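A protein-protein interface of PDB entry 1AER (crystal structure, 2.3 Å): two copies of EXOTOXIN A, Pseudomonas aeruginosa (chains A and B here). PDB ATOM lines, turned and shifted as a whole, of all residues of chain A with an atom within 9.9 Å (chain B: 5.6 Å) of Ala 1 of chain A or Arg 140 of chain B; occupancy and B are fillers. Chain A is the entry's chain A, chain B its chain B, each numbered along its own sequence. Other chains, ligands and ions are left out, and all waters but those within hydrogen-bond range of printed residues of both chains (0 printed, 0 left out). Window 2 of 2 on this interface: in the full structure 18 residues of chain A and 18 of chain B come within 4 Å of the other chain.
The guanidinium group (NE) of Arg 34 of chain A sits at hydrogen-bond distance from the backbone carbonyl oxygen (O) of Leu 141 of chain B, at 3.2 Å.
OD2 of Asp 142 of chain B is in salt-bridge range of NH2 of Arg 34 of chain A (2.8 Å).
A ring nitrogen (ND1) of His 135 of chain B sits at hydrogen-bond distance from the guanidinium group (NE) of Arg 140 of chain B, at 3.2 Å.
NE2 of His 135 of chain B lies within hydrogen-bond range of OD1 of Asp 142 of chain B (3.2 Å).
N of Arg 140 of chain B is in hydrogen-bond range of OD1 of Asp 142 of chain B (2.7 Å).
N of Gly 159 of chain B lies within hydrogen-bond range of O of Asp 142 of chain B (2.7 Å).
Among the printed residues, merely in contact across the chains: Phe 2 of chain A with Leu 141 of chain B (3.3 Å), Ala 1 of chain A with Arg 140 of chain B (3.4 Å) and Phe 2 of chain A with Pro 161 of chain B (3.6 Å).
Ala 1 of chain A touches one residue of chain B.
Of the printed residues of chain B, Phe 2 of chain A touches Leu 141 (3.3 Å) and Pro 161 (3.6 Å).
Gly 7 of chain A touches none of the printed residues of chain B.
Printed residues of chain B within 4 Å of Arg 34 of chain A: Leu 141 and Asp 142.
No residue of chain A comes within 4 Å of Pro 136 of chain B.
No residue of chain A comes within 4 Å of Leu 139 of chain B.
Asp 142 of chain B touches just one residue of chain A: Arg 34 (2.8 Å).
No residue of chain A comes within 4 Å of Gly 159 of chain B.
The nearest residue of chain B that does not touch Ala 1 of chain A is Pro 161 of chain B (4.6 Å).
The nearest printed residue of chain B that does not touch Arg 34 of chain A is His 135 of chain B (5.2 Å).
Along chain B the printed residues that touch a printed residue of chain A span positions 140 to 161.
Hydrophobic or aromatic side chains of chain A within 4 Å of the printed part of chain B: Phe 2.
Among the printed residues, Asp or Glu carboxylates within 4 Å of a Lys or Arg side-chain nitrogen of the other chain: Arg 34 of chain A with Asp 142 of chain B (2.8 Å).
No position is printed for both chains.
Of the 5 pairs that touch across the chains among the printed residues, none has its exchanged pair printed and touching as well.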
ATOM      1  N   ALA A   1     -17.007  27.933   5.855  1.00  0.00           N
ATOM      2  CA  ALA A   1     -15.697  28.076   5.176  1.00  0.00           C
ATOM      3  C   ALA A   1     -15.655  27.187   3.918  1.00  0.00           C
ATOM      4  O   ALA A   1     -16.388  26.191   3.816  1.00  0.00           O
ATOM      5  CB  ALA A   1     -14.552  27.730   6.142  1.00  0.00           C
ATOM      6  N   PHE A   2     -14.831  27.608   2.955  1.00  0.00           N
ATOM      7  CA  PHE A   2     -14.645  26.931   1.673  1.00  0.00           C
ATOM      8  C   PHE A   2     -13.182  26.540   1.395  1.00  0.00           C
ATOM      9  O   PHE A   2     -12.897  25.850   0.426  1.00  0.00           O
ATOM     10  CB  PHE A   2     -15.069  27.878   0.563  1.00  0.00           C
ATOM     11  CG  PHE A   2     -16.435  28.456   0.741  1.00  0.00           C
ATOM     12  CD1 PHE A   2     -17.554  27.635   0.801  1.00  0.00           C
ATOM     13  CD2 PHE A   2     -16.613  29.830   0.765  1.00  0.00           C
ATOM     14  CE1 PHE A   2     -18.834  28.179   0.872  1.00  0.00           C
ATOM     15  CE2 PHE A   2     -17.885  30.376   0.838  1.00  0.00           C
ATOM     16  CZ  PHE A   2     -19.000  29.546   0.888  1.00  0.00           C
ATOM     17  N   LEU A   3     -12.265  26.989   2.240  1.00  0.00           N
ATOM     18  CA  LEU A   3     -10.844  26.732   2.068  1.00  0.00           C
ATOM     19  C   LEU A   3     -10.281  25.511   2.778  1.00  0.00           C
ATOM     20  O   LEU A   3      -9.067  25.347   2.857  1.00  0.00           O
ATOM     21  CB  LEU A   3     -10.060  27.960   2.519  1.00  0.00           C
ATOM     22  CG  LEU A   3     -10.513  29.306   1.961  1.00  0.00           C
ATOM     23  CD1 LEU A   3      -9.531  30.388   2.354  1.00  0.00           C
ATOM     24  CD2 LEU A   3     -10.632  29.219   0.466  1.00  0.00           C
ATOM     25  N   GLY A   4     -11.143  24.676   3.327  1.00  0.00           N
ATOM     26  CA  GLY A   4     -10.675  23.485   4.010  1.00  0.00           C
ATOM     27  C   GLY A   4      -9.886  23.776   5.270  1.00  0.00           C
ATOM     28  O   GLY A   4     -10.055  24.835   5.881  1.00  0.00           O
ATOM     29  N   ASP A   5      -8.993  22.857   5.640  1.00  0.00           N
ATOM     30  CA  ASP A   5      -8.198  23.019   6.855  1.00  0.00           C
ATOM     31  C   ASP A   5      -6.690  23.140   6.680  1.00  0.00           C
ATOM     32  O   ASP A   5      -6.065  22.421   5.875  1.00  0.00           O
ATOM     33  CB  ASP A   5      -8.519  21.908   7.878  1.00  0.00           C
ATOM     34  CG  ASP A   5      -7.960  20.523   7.477  1.00  0.00           C
ATOM     35  OD1 ASP A   5      -6.721  20.313   7.580  1.00  0.00           O
ATOM     36  OD2 ASP A   5      -8.766  19.627   7.110  1.00  0.00           O
ATOM     37  N   GLY A   6      -6.111  24.033   7.480  1.00  0.00           N
ATOM     38  CA  GLY A   6      -4.678  24.244   7.433  1.00  0.00           C
ATOM     39  C   GLY A   6      -4.160  25.657   7.646  1.00  0.00           C
ATOM     40  O   GLY A   6      -3.080  26.000   7.130  1.00  0.00           O
ATOM     41  N   GLY A   7      -4.889  26.482   8.395  1.00  0.00           N
ATOM     42  CA  GLY A   7      -4.401  27.835   8.627  1.00  0.00           C
ATOM     43  C   GLY A   7      -4.888  28.868   7.633  1.00  0.00           C
ATOM     44  O   GLY A   7      -5.527  28.531   6.628  1.00  0.00           O
ATOM     45  N   VAL A   9      -4.986  31.572   4.658  1.00  0.00           N
ATOM     46  CA  VAL A   9      -4.451  31.825   3.353  1.00  0.00           C
ATOM     47  C   VAL A   9      -4.170  33.304   3.141  1.00  0.00           C
ATOM     48  O   VAL A   9      -4.831  34.173   3.705  1.00  0.00           O
ATOM     49  CB  VAL A   9      -5.446  31.310   2.291  1.00  0.00           C
ATOM     50  CG1 VAL A   9      -4.881  31.446   0.910  1.00  0.00           C
ATOM     51  CG2 VAL A   9      -5.792  29.857   2.573  1.00  0.00           C
ATOM     52  N   TRP A  19      -1.606  27.360   1.051  1.00  0.00           N
ATOM     53  CA  TRP A  19      -2.432  26.696   0.072  1.00  0.00           C
ATOM     54  C   TRP A  19      -1.579  25.634  -0.617  1.00  0.00           C
ATOM     55  O   TRP A  19      -0.457  25.920  -1.013  1.00  0.00           O
ATOM     56  CB  TRP A  19      -2.925  27.718  -0.945  1.00  0.00           C
ATOM     57  CG  TRP A  19      -3.958  27.175  -1.742  1.00  0.00           C
ATOM     58  CD1 TRP A  19      -3.862  26.772  -3.023  1.00  0.00           C
ATOM     59  CD2 TRP A  19      -5.250  26.815  -1.287  1.00  0.00           C
ATOM     60  NE1 TRP A  19      -5.021  26.147  -3.402  1.00  0.00           N
ATOM     61  CE2 TRP A  19      -5.898  26.159  -2.350  1.00  0.00           C
ATOM     62  CE3 TRP A  19      -5.928  26.972  -0.069  1.00  0.00           C
ATOM     63  CZ2 TRP A  19      -7.206  25.658  -2.249  1.00  0.00           C
ATOM     64  CZ3 TRP A  19      -7.225  26.476   0.036  1.00  0.00           C
ATOM     65  CH2 TRP A  19      -7.853  25.821  -1.055  1.00  0.00           C
ATOM     66  N   ARG A  23      -4.487  20.602  -0.186  1.00  0.00           N
ATOM     67  CA  ARG A  23      -5.570  21.372   0.450  1.00  0.00           C
ATOM     68  C   ARG A  23      -6.638  21.853  -0.559  1.00  0.00           C
ATOM     69  O   ARG A  23      -7.761  22.186  -0.169  1.00  0.00           O
ATOM     70  CB  ARG A  23      -4.993  22.550   1.247  1.00  0.00           C
ATOM     71  CG  ARG A  23      -6.022  23.329   1.973  1.00  0.00           C
ATOM     72  CD  ARG A  23      -5.409  24.499   2.691  1.00  0.00           C
ATOM     73  NE  ARG A  23      -6.443  25.173   3.457  1.00  0.00           N
ATOM     74  CZ  ARG A  23      -6.219  26.164   4.307  1.00  0.00           C
ATOM     75  NH1 ARG A  23      -4.998  26.627   4.463  1.00  0.00           N
ATOM     76  NH2 ARG A  23      -7.221  26.703   4.984  1.00  0.00           N
ATOM     77  N   GLN A  26      -9.135  18.842  -1.183  1.00  0.00           N
ATOM     78  CA  GLN A  26     -10.062  18.736  -0.082  1.00  0.00           C
ATOM     79  C   GLN A  26     -11.194  19.739  -0.281  1.00  0.00           C
ATOM     80  O   GLN A  26     -12.350  19.374  -0.343  1.00  0.00           O
ATOM     81  CB  GLN A  26      -9.299  19.039   1.200  1.00  0.00           C
ATOM     82  CG  GLN A  26      -9.968  18.534   2.449  1.00  0.00           C
ATOM     83  CD  GLN A  26      -9.294  19.059   3.684  1.00  0.00           C
ATOM     84  OE1 GLN A  26      -9.553  20.185   4.118  1.00  0.00           O
ATOM     85  NE2 GLN A  26      -8.382  18.270   4.235  1.00  0.00           N
ATOM     86  N   ALA A  27     -10.857  21.009  -0.389  1.00  0.00           N
ATOM     87  CA  ALA A  27     -11.847  22.071  -0.606  1.00  0.00           C
ATOM     88  C   ALA A  27     -12.719  21.761  -1.806  1.00  0.00           C
ATOM     89  O   ALA A  27     -13.931  21.931  -1.751  1.00  0.00           O
ATOM     90  CB  ALA A  27     -11.154  23.438  -0.775  1.00  0.00           C
ATOM     91  N   HIS A  28     -12.101  21.249  -2.870  1.00  0.00           N
ATOM     92  CA  HIS A  28     -12.807  20.867  -4.086  1.00  0.00           C
ATOM     93  C   HIS A  28     -13.907  19.834  -3.819  1.00  0.00           C
ATOM     94  O   HIS A  28     -15.076  20.020  -4.226  1.00  0.00           O
ATOM     95  CB  HIS A  28     -11.824  20.296  -5.111  1.00  0.00           C
ATOM     96  CG  HIS A  28     -12.461  19.946  -6.416  1.00  0.00           C
ATOM     97  ND1 HIS A  28     -12.746  20.886  -7.384  1.00  0.00           N
ATOM     98  CD2 HIS A  28     -12.896  18.761  -6.901  1.00  0.00           C
ATOM     99  CE1 HIS A  28     -13.329  20.299  -8.412  1.00  0.00           C
ATOM    100  NE2 HIS A  28     -13.433  19.008  -8.143  1.00  0.00           N
ATOM    101  N   GLN A  30     -15.169  19.015  -0.957  1.00  0.00           N
ATOM    102  CA  GLN A  30     -16.187  19.534  -0.050  1.00  0.00           C
ATOM    103  C   GLN A  30     -17.202  20.335  -0.882  1.00  0.00           C
ATOM    104  O   GLN A  30     -18.390  20.231  -0.658  1.00  0.00           O
ATOM    105  CB  GLN A  30     -15.573  20.427   1.034  1.00  0.00           C
ATOM    106  CG  GLN A  30     -14.439  19.785   1.857  1.00  0.00           C
ATOM    107  CD  GLN A  30     -13.785  20.734   2.920  1.00  0.00           C
ATOM    108  OE1 GLN A  30     -12.870  20.321   3.648  1.00  0.00           O
ATOM    109  NE2 GLN A  30     -14.251  21.989   3.002  1.00  0.00           N
ATOM    110  N   LEU A  31     -16.746  21.096  -1.871  1.00  0.00           N
ATOM    111  CA  LEU A  31     -17.657  21.898  -2.711  1.00  0.00           C
ATOM    112  C   LEU A  31     -18.530  21.037  -3.581  1.00  0.00           C
ATOM    113  O   LEU A  31     -19.658  21.399  -3.881  1.00  0.00           O
ATOM    114  CB  LEU A  31     -16.891  22.859  -3.618  1.00  0.00           C
ATOM    115  CG  LEU A  31     -16.378  24.035  -2.820  1.00  0.00           C
ATOM    116  CD1 LEU A  31     -15.538  24.913  -3.656  1.00  0.00           C
ATOM    117  CD2 LEU A  31     -17.562  24.780  -2.297  1.00  0.00           C
ATOM    118  N   GLU A  33     -19.625  18.019  -2.886  1.00  0.00           N
ATOM    119  CA  GLU A  33     -20.674  17.438  -2.077  1.00  0.00           C
ATOM    120  C   GLU A  33     -21.780  18.420  -1.777  1.00  0.00           C
ATOM    121  O   GLU A  33     -22.915  18.026  -1.559  1.00  0.00           O
ATOM    122  CB  GLU A  33     -20.089  16.878  -0.801  1.00  0.00           C
ATOM    123  CG  GLU A  33     -19.281  15.646  -1.087  1.00  0.00           C
ATOM    124  CD  GLU A  33     -18.482  15.178   0.096  1.00  0.00           C
ATOM    125  OE1 GLU A  33     -18.317  15.942   1.089  1.00  0.00           O
ATOM    126  OE2 GLU A  33     -18.010  14.022   0.016  1.00  0.00           O
ATOM    127  N   ARG A  34     -21.462  19.703  -1.734  1.00  0.00           N
ATOM    128  CA  ARG A  34     -22.493  20.706  -1.485  1.00  0.00           C
ATOM    129  C   ARG A  34     -23.113  21.179  -2.822  1.00  0.00           C
ATOM    130  O   ARG A  34     -23.725  22.249  -2.898  1.00  0.00           O
ATOM    131  CB  ARG A  34     -21.914  21.862  -0.679  1.00  0.00           C
ATOM    132  CG  ARG A  34     -21.789  21.525   0.758  1.00  0.00           C
ATOM    133  CD  ARG A  34     -23.182  21.105   1.251  1.00  0.00           C
ATOM    134  NE  ARG A  34     -23.218  20.806   2.672  1.00  0.00           N
ATOM    135  CZ  ARG A  34     -23.019  19.600   3.183  1.00  0.00           C
ATOM    136  NH1 ARG A  34     -22.828  18.570   2.373  1.00  0.00           N
ATOM    137  NH2 ARG A  34     -23.052  19.409   4.504  1.00  0.00           N
ATOM    138  N   TYR A  36     -21.590  22.232  -5.848  1.00  0.00           N
ATOM    139  CA  TYR A  36     -20.954  23.213  -6.702  1.00  0.00           C
ATOM    140  C   TYR A  36     -20.107  22.554  -7.773  1.00  0.00           C
ATOM    141  O   TYR A  36     -19.552  21.469  -7.564  1.00  0.00           O
ATOM    142  CB  TYR A  36     -20.110  24.172  -5.914  1.00  0.00           C
ATOM    143  CG  TYR A  36     -20.940  25.197  -5.225  1.00  0.00           C
ATOM    144  CD1 TYR A  36     -21.720  24.849  -4.114  1.00  0.00           C
ATOM    145  CD2 TYR A  36     -21.047  26.501  -5.725  1.00  0.00           C
ATOM    146  CE1 TYR A  36     -22.596  25.757  -3.528  1.00  0.00           C
ATOM    147  CE2 TYR A  36     -21.924  27.430  -5.135  1.00  0.00           C
ATOM    148  CZ  TYR A  36     -22.690  27.041  -4.043  1.00  0.00           C
ATOM    149  OH  TYR A  36     -23.553  27.912  -3.434  1.00  0.00           O
ATOM    150  N   VAL A  53     -11.534  36.407  -2.652  1.00  0.00           N
ATOM    151  CA  VAL A  53     -11.576  35.180  -1.862  1.00  0.00           C
ATOM    152  C   VAL A  53     -12.182  35.412  -0.485  1.00  0.00           C
ATOM    153  O   VAL A  53     -13.075  34.676  -0.111  1.00  0.00           O
ATOM    154  CB  VAL A  53     -10.189  34.484  -1.774  1.00  0.00           C
ATOM    155  CG1 VAL A  53     -10.158  33.406  -0.686  1.00  0.00           C
ATOM    156  CG2 VAL A  53      -9.874  33.843  -3.098  1.00  0.00           C
ATOM    157  N   PHE A  54     -11.789  36.471   0.224  1.00  0.00           N
ATOM    158  CA  PHE A  54     -12.336  36.727   1.554  1.00  0.00           C
ATOM    159  C   PHE A  54     -13.238  37.941   1.588  1.00  0.00           C
ATOM    160  O   PHE A  54     -13.039  38.825   2.431  1.00  0.00           O
ATOM    161  CB  PHE A  54     -11.215  36.970   2.558  1.00  0.00           C
ATOM    162  CG  PHE A  54     -10.091  36.000   2.458  1.00  0.00           C
ATOM    163  CD1 PHE A  54      -9.091  36.167   1.500  1.00  0.00           C
ATOM    164  CD2 PHE A  54     -10.015  34.914   3.323  1.00  0.00           C
ATOM    165  CE1 PHE A  54      -8.025  35.258   1.408  1.00  0.00           C
ATOM    166  CE2 PHE A  54      -8.956  34.006   3.236  1.00  0.00           C
ATOM    167  CZ  PHE A  54      -7.965  34.178   2.280  1.00  0.00           C
ATOM    168  N   VAL A 167     -18.516  30.625  -5.525  1.00  0.00           N
ATOM    169  CA  VAL A 167     -17.601  30.354  -4.415  1.00  0.00           C
ATOM    170  C   VAL A 167     -16.264  30.424  -5.180  1.00  0.00           C
ATOM    171  O   VAL A 167     -16.150  29.892  -6.285  1.00  0.00           O
ATOM    172  CB  VAL A 167     -17.782  28.933  -3.812  1.00  0.00           C
ATOM    173  CG1 VAL A 167     -16.619  28.615  -2.864  1.00  0.00           C
ATOM    174  CG2 VAL A 167     -19.121  28.835  -3.066  1.00  0.00           C
ATOM    175  N   VAL A 168     -15.295  31.161  -4.666  1.00  0.00           N
ATOM    176  CA  VAL A 168     -14.003  31.276  -5.328  1.00  0.00           C
ATOM    177  C   VAL A 168     -12.898  30.818  -4.345  1.00  0.00           C
ATOM    178  O   VAL A 168     -12.873  31.234  -3.179  1.00  0.00           O
ATOM    179  CB  VAL A 168     -13.777  32.720  -5.832  1.00  0.00           C
ATOM    180  CG1 VAL A 168     -12.449  32.839  -6.574  1.00  0.00           C
ATOM    181  CG2 VAL A 168     -14.897  33.131  -6.758  1.00  0.00           C
ATOM    182  N   ILE A 169     -12.032  29.908  -4.777  1.00  0.00           N
ATOM    183  CA  ILE A 169     -10.962  29.437  -3.902  1.00  0.00           C
ATOM    184  C   ILE A 169      -9.675  29.631  -4.689  1.00  0.00           C
ATOM    185  O   ILE A 169      -9.708  29.784  -5.919  1.00  0.00           O
ATOM    186  CB  ILE A 169     -11.113  27.933  -3.429  1.00  0.00           C
ATOM    187  CG1 ILE A 169     -10.980  26.939  -4.584  1.00  0.00           C
ATOM    188  CG2 ILE A 169     -12.436  27.727  -2.746  1.00  0.00           C
ATOM    189  CD1 ILE A 169     -11.130  25.449  -4.184  1.00  0.00           C
ATOM    190  N   HIS B 135     -19.360  18.537  10.276  1.00  0.00           N
ATOM    191  CA  HIS B 135     -18.242  19.382  10.700  1.00  0.00           C
ATOM    192  C   HIS B 135     -18.724  20.153  11.899  1.00  0.00           C
ATOM    193  O   HIS B 135     -19.905  20.176  12.187  1.00  0.00           O
ATOM    194  CB  HIS B 135     -17.866  20.384   9.604  1.00  0.00           C
ATOM    195  CG  HIS B 135     -18.988  21.294   9.221  1.00  0.00           C
ATOM    196  ND1 HIS B 135     -19.197  22.517   9.822  1.00  0.00           N
ATOM    197  CD2 HIS B 135     -19.991  21.132   8.329  1.00  0.00           C
ATOM    198  CE1 HIS B 135     -20.287  23.068   9.324  1.00  0.00           C
ATOM    199  NE2 HIS B 135     -20.786  22.247   8.413  1.00  0.00           N
ATOM    200  N   PRO B 136     -17.812  20.778  12.628  1.00  0.00           N
ATOM    201  CA  PRO B 136     -18.259  21.529  13.790  1.00  0.00           C
ATOM    202  C   PRO B 136     -19.117  22.700  13.379  1.00  0.00           C
ATOM    203  O   PRO B 136     -18.953  23.251  12.280  1.00  0.00           O
ATOM    204  CB  PRO B 136     -16.951  22.033  14.388  1.00  0.00           C
ATOM    205  CG  PRO B 136     -15.997  20.950  14.032  1.00  0.00           C
ATOM    206  CD  PRO B 136     -16.352  20.617  12.623  1.00  0.00           C
ATOM    207  N   PRO B 138     -20.226  26.569  13.476  1.00  0.00           N
ATOM    208  CA  PRO B 138     -21.477  26.857  12.788  1.00  0.00           C
ATOM    209  C   PRO B 138     -21.637  26.308  11.395  1.00  0.00           C
ATOM    210  O   PRO B 138     -20.719  25.724  10.812  1.00  0.00           O
ATOM    211  CB  PRO B 138     -21.544  28.380  12.820  1.00  0.00           C
ATOM    212  CG  PRO B 138     -20.190  28.784  12.745  1.00  0.00           C
ATOM    213  CD  PRO B 138     -19.432  27.795  13.612  1.00  0.00           C
ATOM    214  N   LEU B 139     -22.891  26.379  10.961  1.00  0.00           N
ATOM    215  CA  LEU B 139     -23.369  25.945   9.659  1.00  0.00           C
ATOM    216  C   LEU B 139     -22.559  26.732   8.638  1.00  0.00           C
ATOM    217  O   LEU B 139     -22.213  27.876   8.896  1.00  0.00           O
ATOM    218  CB  LEU B 139     -24.834  26.356   9.518  1.00  0.00           C
ATOM    219  CG  LEU B 139     -26.068  25.524   9.858  1.00  0.00           C
ATOM    220  CD1 LEU B 139     -25.738  24.203  10.445  1.00  0.00           C
ATOM    221  CD2 LEU B 139     -26.969  26.347  10.726  1.00  0.00           C
ATOM    222  N   ARG B 140     -22.279  26.137   7.481  1.00  0.00           N
ATOM    223  CA  ARG B 140     -21.534  26.803   6.421  1.00  0.00           C
ATOM    224  C   ARG B 140     -22.484  26.707   5.271  1.00  0.00           C
ATOM    225  O   ARG B 140     -23.524  27.371   5.266  1.00  0.00           O
ATOM    226  CB  ARG B 140     -20.264  26.034   6.117  1.00  0.00           C
ATOM    227  CG  ARG B 140     -19.391  25.908   7.300  1.00  0.00           C
ATOM    228  CD  ARG B 140     -18.340  24.880   7.093  1.00  0.00           C
ATOM    229  NE  ARG B 140     -17.520  24.778   8.296  1.00  0.00           N
ATOM    230  CZ  ARG B 140     -16.580  23.861   8.494  1.00  0.00           C
ATOM    231  NH1 ARG B 140     -16.308  22.949   7.564  1.00  0.00           N
ATOM    232  NH2 ARG B 140     -15.902  23.865   9.627  1.00  0.00           N
ATOM    233  N   LEU B 141     -22.174  25.844   4.318  1.00  0.00           N
ATOM    234  CA  LEU B 141     -23.084  25.649   3.203  1.00  0.00           C
ATOM    235  C   LEU B 141     -24.168  24.613   3.568  1.00  0.00           C
ATOM    236  O   LEU B 141     -24.479  23.720   2.778  1.00  0.00           O
ATOM    237  CB  LEU B 141     -22.325  25.212   1.943  1.00  0.00           C
ATOM    238  CG  LEU B 141     -21.542  26.259   1.157  1.00  0.00           C
ATOM    239  CD1 LEU B 141     -20.818  25.488   0.103  1.00  0.00           C
ATOM    240  CD2 LEU B 141     -22.471  27.336   0.534  1.00  0.00           C
ATOM    241  N   ASP B 142     -24.707  24.686   4.780  1.00  0.00           N
ATOM    242  CA  ASP B 142     -25.762  23.771   5.194  1.00  0.00           C
ATOM    243  C   ASP B 142     -26.934  24.523   5.825  1.00  0.00           C
ATOM    244  O   ASP B 142     -26.883  25.752   6.001  1.00  0.00           O
ATOM    245  CB  ASP B 142     -25.286  22.692   6.177  1.00  0.00           C
ATOM    246  CG  ASP B 142     -23.818  22.727   6.454  1.00  0.00           C
ATOM    247  OD1 ASP B 142     -23.334  23.638   7.148  1.00  0.00           O
ATOM    248  OD2 ASP B 142     -23.141  21.771   6.059  1.00  0.00           O
ATOM    249  N   LEU B 158     -30.218  28.834   7.900  1.00  0.00           N
ATOM    250  CA  LEU B 158     -29.324  28.603   6.782  1.00  0.00           C
ATOM    251  C   LEU B 158     -27.945  29.082   7.215  1.00  0.00           C
ATOM    252  O   LEU B 158     -27.824  30.127   7.853  1.00  0.00           O
ATOM    253  CB  LEU B 158     -29.772  29.412   5.566  1.00  0.00           C
ATOM    254  CG  LEU B 158     -31.223  29.325   5.115  1.00  0.00           C
ATOM    255  CD1 LEU B 158     -31.407  30.220   3.882  1.00  0.00           C
ATOM    256  CD2 LEU B 158     -31.560  27.898   4.809  1.00  0.00           C
ATOM    257  N   GLY B 159     -26.914  28.291   6.978  1.00  0.00           N
ATOM    258  CA  GLY B 159     -25.600  28.756   7.337  1.00  0.00           C
ATOM    259  C   GLY B 159     -25.451  30.038   6.541  1.00  0.00           C
ATOM    260  O   GLY B 159     -26.045  30.179   5.463  1.00  0.00           O
ATOM    261  N   TRP B 160     -24.737  31.007   7.089  1.00  0.00           N
ATOM    262  CA  TRP B 160     -24.539  32.268   6.409  1.00  0.00           C
ATOM    263  C   TRP B 160     -23.953  32.187   4.977  1.00  0.00           C
ATOM    264  O   TRP B 160     -24.317  33.002   4.118  1.00  0.00           O
ATOM    265  CB  TRP B 160     -23.740  33.209   7.291  1.00  0.00           C
ATOM    266  CG  TRP B 160     -24.571  33.910   8.232  1.00  0.00           C
ATOM    267  CD1 TRP B 160     -24.468  33.869   9.578  1.00  0.00           C
ATOM    268  CD2 TRP B 160     -25.638  34.814   7.932  1.00  0.00           C
ATOM    269  NE1 TRP B 160     -25.396  34.698  10.152  1.00  0.00           N
ATOM    270  CE2 TRP B 160     -26.138  35.293   9.165  1.00  0.00           C
ATOM    271  CE3 TRP B 160     -26.216  35.277   6.745  1.00  0.00           C
ATOM    272  CZ2 TRP B 160     -27.200  36.211   9.256  1.00  0.00           C
ATOM    273  CZ3 TRP B 160     -27.265  36.192   6.825  1.00  0.00           C
ATOM    274  CH2 TRP B 160     -27.748  36.651   8.084  1.00  0.00           C
ATOM    275  N   PRO B 161     -22.978  31.298   4.731  1.00  0.00           N
ATOM    276  CA  PRO B 161     -22.426  31.187   3.388  1.00  0.00           C
ATOM    277  C   PRO B 161     -23.544  30.821   2.425  1.00  0.00           C
ATOM    278  O   PRO B 161     -23.523  31.275   1.290  1.00  0.00           O
ATOM    279  CB  PRO B 161     -21.453  30.042   3.530  1.00  0.00           C
ATOM    280  CG  PRO B 161     -20.916  30.243   4.853  1.00  0.00           C
ATOM    281  CD  PRO B 161     -22.159  30.524   5.666  1.00  0.00           C
ATOM    282  N   LEU B 162     -24.532  30.029   2.874  1.00  0.00           N
ATOM    283  CA  LEU B 162     -25.681  29.649   2.037  1.00  0.00           C
ATOM    284  C   LEU B 162     -26.672  30.808   2.015  1.00  0.00           C
ATOM    285  O   LEU B 162     -27.210  31.175   0.960  1.00  0.00           O
ATOM    286  CB  LEU B 162     -26.362  28.403   2.604  1.00  0.00           C
ATOM    287  CG  LEU B 162     -27.568  27.952   1.776  1.00  0.00           C
ATOM    288  CD1 LEU B 162     -27.206  27.609   0.330  1.00  0.00           C
ATOM    289  CD2 LEU B 162     -28.248  26.704   2.340  1.00  0.00           C
